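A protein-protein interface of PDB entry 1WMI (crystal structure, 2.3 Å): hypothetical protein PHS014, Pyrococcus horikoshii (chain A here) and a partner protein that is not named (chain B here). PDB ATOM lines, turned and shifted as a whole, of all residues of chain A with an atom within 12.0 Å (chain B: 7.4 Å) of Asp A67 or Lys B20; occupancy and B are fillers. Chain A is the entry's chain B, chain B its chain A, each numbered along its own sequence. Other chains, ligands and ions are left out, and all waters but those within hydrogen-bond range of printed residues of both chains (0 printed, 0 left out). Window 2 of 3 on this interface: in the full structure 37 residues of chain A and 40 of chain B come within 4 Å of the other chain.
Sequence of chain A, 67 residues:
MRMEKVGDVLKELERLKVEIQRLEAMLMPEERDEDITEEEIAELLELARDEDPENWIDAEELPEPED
The side-chain hydroxyl (OH) of Tyr B23 sits at hydrogen-bond distance from the backbone carbonyl oxygen (O) of Pro A63 (2.9 Å). The side-chain carboxylate (OD2) of Asp A67 lies within salt-bridge range of the guanidinium group (NH1) of Arg B24, at 3.999 Å.
Leu A62 touches Tyr B23 (CB to OH, 3.6 Å). CD1 of Leu A62 touches CE1 of Phe B26, at 3.5 Å. Glu A66 touches Lys B20. Lys B20 touches Asp A67 (NZ to CB, 3.1 Å).
Printed residues of chain B within 4 Å of Asp A67: Lys B20 (3.1 Å) and Arg B24 (3.999 Å). Lys B20 touches two residues of chain A. No residue of chain A comes within 4 Å of Pro B19. No residue of chain A comes within 4 Å of Ala B21. No residue of chain A comes within 4 Å of His B22. Of the printed residues of chain A, Arg B24 touches Asp A67. Of the printed residues of chain B, Leu A62 touches Tyr B23 (3.6 Å) and Phe B26 (3.5 Å). Of the printed residues of chain B, Glu A66 touches Lys B20 (3.6 Å). Printed residues of chain A within 4 Å of Tyr B23: Leu A62 and Pro A63. Printed residues of chain B within 4 Å of Pro A63: Tyr B23. Leu B18 touches none of the printed residues of chain A. Ser B17 touches none of the printed residues of chain A. The nearest printed residue of chain B that does not touch Asp A67 is Ala B21 (8.4 Å). The nearest residue of chain A that does not touch Lys B20 is Pro A65 (5.0 Å). The nearest printed residue of chain B that does not touch Leu A62 is Arg B24 (8.8 Å).
Of the 10 printed residues of chain B, 4 touch a printed residue of chain A. Hydrophobic or aromatic side chains of chain B within 4 Å of the printed part of chain A: Tyr B23 and Phe B26. Of the 6 printed residues of chain A, 4 touch a printed residue of chain B. Printed residues of chain A that touch a printed residue of chain B: Leu A62, Pro A63, Glu A66 and Asp A67. Among the printed residues, Asp or Glu carboxylates within 4 Å of a Lys or Arg side-chain nitrogen of the other chain: Asp A67 with Arg B24 (3.999 Å).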
ATOM      1  N   LEU A  62       7.698  12.147 -14.898  1.00  0.00           N
ATOM      2  CA  LEU A  62       8.763  12.572 -15.797  1.00  0.00           C
ATOM      3  C   LEU A  62       9.969  12.875 -14.921  1.00  0.00           C
ATOM      4  O   LEU A  62       9.834  13.298 -13.773  1.00  0.00           O
ATOM      5  CB  LEU A  62       8.387  13.846 -16.564  1.00  0.00           C
ATOM      6  CG  LEU A  62       7.517  13.847 -17.821  1.00  0.00           C
ATOM      7  CD1 LEU A  62       7.235  15.279 -18.209  1.00  0.00           C
ATOM      8  CD2 LEU A  62       8.217  13.143 -18.957  1.00  0.00           C
ATOM      9  N   PRO A  63      11.172  12.674 -15.461  1.00  0.00           N
ATOM     10  CA  PRO A  63      12.414  12.925 -14.732  1.00  0.00           C
ATOM     11  C   PRO A  63      12.580  14.361 -14.228  1.00  0.00           C
ATOM     12  O   PRO A  63      11.915  15.276 -14.692  1.00  0.00           O
ATOM     13  CB  PRO A  63      13.478  12.559 -15.753  1.00  0.00           C
ATOM     14  CG  PRO A  63      12.817  11.484 -16.545  1.00  0.00           C
ATOM     15  CD  PRO A  63      11.456  12.072 -16.774  1.00  0.00           C
ATOM     16  N   GLU A  64      13.503  14.547 -13.291  1.00  0.00           N
ATOM     17  CA  GLU A  64      13.797  15.856 -12.685  1.00  0.00           C
ATOM     18  C   GLU A  64      15.242  16.299 -13.022  1.00  0.00           C
ATOM     19  O   GLU A  64      16.169  15.566 -12.704  1.00  0.00           O
ATOM     20  CB  GLU A  64      13.656  15.714 -11.167  1.00  0.00           C
ATOM     21  CG  GLU A  64      13.274  14.294 -10.718  1.00  0.00           C
ATOM     22  CD  GLU A  64      14.178  13.748  -9.630  1.00  0.00           C
ATOM     23  OE1 GLU A  64      14.136  14.264  -8.488  1.00  0.00           O
ATOM     24  OE2 GLU A  64      14.932  12.795  -9.926  1.00  0.00           O
ATOM     25  N   PRO A  65      15.454  17.487 -13.649  1.00  0.00           N
ATOM     26  CA  PRO A  65      16.802  17.963 -14.000  1.00  0.00           C
ATOM     27  C   PRO A  65      18.065  17.472 -13.262  1.00  0.00           C
ATOM     28  O   PRO A  65      18.185  17.552 -12.028  1.00  0.00           O
ATOM     29  CB  PRO A  65      16.622  19.474 -13.986  1.00  0.00           C
ATOM     30  CG  PRO A  65      15.350  19.588 -14.777  1.00  0.00           C
ATOM     31  CD  PRO A  65      14.455  18.465 -14.141  1.00  0.00           C
ATOM     32  N   GLU A  66      18.983  16.970 -14.099  1.00  0.00           N
ATOM     33  CA  GLU A  66      20.279  16.399 -13.754  1.00  0.00           C
ATOM     34  C   GLU A  66      21.261  17.351 -13.090  1.00  0.00           C
ATOM     35  O   GLU A  66      21.782  17.024 -12.026  1.00  0.00           O
ATOM     36  CB  GLU A  66      20.911  15.757 -15.007  1.00  0.00           C
ATOM     37  CG  GLU A  66      20.970  16.608 -16.271  1.00  0.00           C
ATOM     38  CD  GLU A  66      21.229  15.733 -17.487  1.00  0.00           C
ATOM     39  OE1 GLU A  66      20.730  14.578 -17.507  1.00  0.00           O
ATOM     40  OE2 GLU A  66      21.913  16.199 -18.423  1.00  0.00           O
ATOM     41  N   ASP A  67      21.502  18.508 -13.707  1.00  0.00           N
ATOM     42  CA  ASP A  67      22.412  19.541 -13.177  1.00  0.00           C
ATOM     43  C   ASP A  67      22.876  19.367 -11.721  1.00  0.00           C
ATOM     44  O   ASP A  67      22.565  20.234 -10.868  1.00  0.00           O
ATOM     45  CB  ASP A  67      21.767  20.927 -13.339  1.00  0.00           C
ATOM     46  CG  ASP A  67      20.619  21.160 -12.366  1.00  0.00           C
ATOM     47  OD1 ASP A  67      20.022  20.159 -11.911  1.00  0.00           O
ATOM     48  OD2 ASP A  67      20.317  22.336 -12.060  1.00  0.00           O
ATOM     49  OXT ASP A  67      23.549  18.352 -11.451  1.00  0.00           O
ATOM     50  N   SER B  17      15.488  14.914 -26.788  1.00  0.00           N
ATOM     51  CA  SER B  17      16.373  15.574 -27.742  1.00  0.00           C
ATOM     52  C   SER B  17      16.576  17.021 -27.332  1.00  0.00           C
ATOM     53  O   SER B  17      17.426  17.722 -27.872  1.00  0.00           O
ATOM     54  CB  SER B  17      15.763  15.533 -29.145  1.00  0.00           C
ATOM     55  OG  SER B  17      15.580  14.205 -29.600  1.00  0.00           O
ATOM     56  N   LEU B  18      15.791  17.465 -26.360  1.00  0.00           N
ATOM     57  CA  LEU B  18      15.874  18.840 -25.898  1.00  0.00           C
ATOM     58  C   LEU B  18      16.976  19.142 -24.900  1.00  0.00           C
ATOM     59  O   LEU B  18      17.343  18.303 -24.070  1.00  0.00           O
ATOM     60  CB  LEU B  18      14.539  19.281 -25.290  1.00  0.00           C
ATOM     61  CG  LEU B  18      13.448  19.778 -26.243  1.00  0.00           C
ATOM     62  CD1 LEU B  18      13.268  18.793 -27.393  1.00  0.00           C
ATOM     63  CD2 LEU B  18      12.148  19.967 -25.464  1.00  0.00           C
ATOM     64  N   PRO B  19      17.517  20.366 -24.978  1.00  0.00           N
ATOM     65  CA  PRO B  19      18.577  20.835 -24.089  1.00  0.00           C
ATOM     66  C   PRO B  19      17.999  20.843 -22.670  1.00  0.00           C
ATOM     67  O   PRO B  19      16.798  21.031 -22.488  1.00  0.00           O
ATOM     68  CB  PRO B  19      18.848  22.248 -24.599  1.00  0.00           C
ATOM     69  CG  PRO B  19      18.472  22.171 -26.047  1.00  0.00           C
ATOM     70  CD  PRO B  19      17.206  21.378 -26.001  1.00  0.00           C
ATOM     71  N   LYS B  20      18.852  20.631 -21.677  1.00  0.00           N
ATOM     72  CA  LYS B  20      18.432  20.619 -20.281  1.00  0.00           C
ATOM     73  C   LYS B  20      17.446  21.774 -20.032  1.00  0.00           C
ATOM     74  O   LYS B  20      16.358  21.578 -19.483  1.00  0.00           O
ATOM     75  CB  LYS B  20      19.679  20.758 -19.398  1.00  0.00           C
ATOM     76  CG  LYS B  20      19.526  20.330 -17.953  1.00  0.00           C
ATOM     77  CD  LYS B  20      20.900  20.044 -17.340  1.00  0.00           C
ATOM     78  CE  LYS B  20      21.794  21.286 -17.269  1.00  0.00           C
ATOM     79  NZ  LYS B  20      21.422  22.215 -16.159  1.00  0.00           N
ATOM     80  N   ALA B  21      17.827  22.971 -20.470  1.00  0.00           N
ATOM     81  CA  ALA B  21      17.014  24.174 -20.312  1.00  0.00           C
ATOM     82  C   ALA B  21      15.594  24.052 -20.859  1.00  0.00           C
ATOM     83  O   ALA B  21      14.634  24.405 -20.175  1.00  0.00           O
ATOM     84  CB  ALA B  21      17.710  25.358 -20.977  1.00  0.00           C
ATOM     85  N   HIS B  22      15.461  23.575 -22.094  1.00  0.00           N
ATOM     86  CA  HIS B  22      14.146  23.424 -22.715  1.00  0.00           C
ATOM     87  C   HIS B  22      13.274  22.418 -21.970  1.00  0.00           C
ATOM     88  O   HIS B  22      12.060  22.597 -21.842  1.00  0.00           O
ATOM     89  CB  HIS B  22      14.297  22.983 -24.170  1.00  0.00           C
ATOM     90  CG  HIS B  22      14.870  24.039 -25.066  1.00  0.00           C
ATOM     91  ND1 HIS B  22      16.133  24.567 -24.878  1.00  0.00           N
ATOM     92  CD2 HIS B  22      14.354  24.657 -26.148  1.00  0.00           C
ATOM     93  CE1 HIS B  22      16.365  25.467 -25.818  1.00  0.00           C
ATOM     94  NE2 HIS B  22      15.308  25.544 -26.601  1.00  0.00           N
ATOM     95  N   TYR B  23      13.898  21.353 -21.494  1.00  0.00           N
ATOM     96  CA  TYR B  23      13.181  20.325 -20.764  1.00  0.00           C
ATOM     97  C   TYR B  23      12.602  20.919 -19.489  1.00  0.00           C
ATOM     98  O   TYR B  23      11.458  20.652 -19.130  1.00  0.00           O
ATOM     99  CB  TYR B  23      14.128  19.186 -20.411  1.00  0.00           C
ATOM    100  CG  TYR B  23      13.467  18.081 -19.642  1.00  0.00           C
ATOM    101  CD1 TYR B  23      12.455  17.323 -20.218  1.00  0.00           C
ATOM    102  CD2 TYR B  23      13.858  17.786 -18.336  1.00  0.00           C
ATOM    103  CE1 TYR B  23      11.843  16.298 -19.519  1.00  0.00           C
ATOM    104  CE2 TYR B  23      13.251  16.762 -17.628  1.00  0.00           C
ATOM    105  CZ  TYR B  23      12.245  16.020 -18.231  1.00  0.00           C
ATOM    106  OH  TYR B  23      11.639  14.995 -17.548  1.00  0.00           O
ATOM    107  N   ARG B  24      13.407  21.730 -18.813  1.00  0.00           N
ATOM    108  CA  ARG B  24      13.005  22.384 -17.573  1.00  0.00           C
ATOM    109  C   ARG B  24      11.745  23.224 -17.804  1.00  0.00           C
ATOM    110  O   ARG B  24      10.822  23.228 -16.984  1.00  0.00           O
ATOM    111  CB  ARG B  24      14.159  23.263 -17.087  1.00  0.00           C
ATOM    112  CG  ARG B  24      14.049  23.772 -15.665  1.00  0.00           C
ATOM    113  CD  ARG B  24      15.336  24.482 -15.283  1.00  0.00           C
ATOM    114  NE  ARG B  24      16.470  23.566 -15.185  1.00  0.00           N
ATOM    115  CZ  ARG B  24      17.636  23.739 -15.802  1.00  0.00           C
ATOM    116  NH1 ARG B  24      18.608  22.851 -15.639  1.00  0.00           N
ATOM    117  NH2 ARG B  24      17.828  24.788 -16.594  1.00  0.00           N
ATOM    118  N   ARG B  25      11.711  23.908 -18.940  1.00  0.00           N
ATOM    119  CA  ARG B  25      10.590  24.766 -19.320  1.00  0.00           C
ATOM    120  C   ARG B  25       9.329  23.925 -19.526  1.00  0.00           C
ATOM    121  O   ARG B  25       8.212  24.341 -19.187  1.00  0.00           O
ATOM    122  CB  ARG B  25      10.939  25.516 -20.616  1.00  0.00           C
ATOM    123  CG  ARG B  25      10.302  26.900 -20.760  1.00  0.00           C
ATOM    124  CD  ARG B  25      10.662  27.513 -22.111  1.00  0.00           C
ATOM    125  NE  ARG B  25      12.103  27.467 -22.362  1.00  0.00           N
ATOM    126  CZ  ARG B  25      12.977  28.365 -21.920  1.00  0.00           C
ATOM    127  NH1 ARG B  25      14.272  28.231 -22.194  1.00  0.00           N
ATOM    128  NH2 ARG B  25      12.557  29.409 -21.224  1.00  0.00           N
ATOM    129  N   PHE B  26       9.518  22.733 -20.080  1.00  0.00           N
ATOM    130  CA  PHE B  26       8.399  21.838 -20.320  1.00  0.00           C
ATOM    131  C   PHE B  26       7.781  21.425 -18.992  1.00  0.00           C
ATOM    132  O   PHE B  26       6.557  21.388 -18.856  1.00  0.00           O
ATOM    133  CB  PHE B  26       8.854  20.602 -21.103  1.00  0.00           C
ATOM    134  CG  PHE B  26       7.755  19.612 -21.349  1.00  0.00           C
ATOM    135  CD1 PHE B  26       7.480  18.607 -20.428  1.00  0.00           C
ATOM    136  CD2 PHE B  26       6.964  19.708 -22.484  1.00  0.00           C
ATOM    137  CE1 PHE B  26       6.424  17.710 -20.644  1.00  0.00           C
ATOM    138  CE2 PHE B  26       5.914  18.823 -22.702  1.00  0.00           C
ATOM    139  CZ  PHE B  26       5.644  17.825 -21.784  1.00  0.00           C
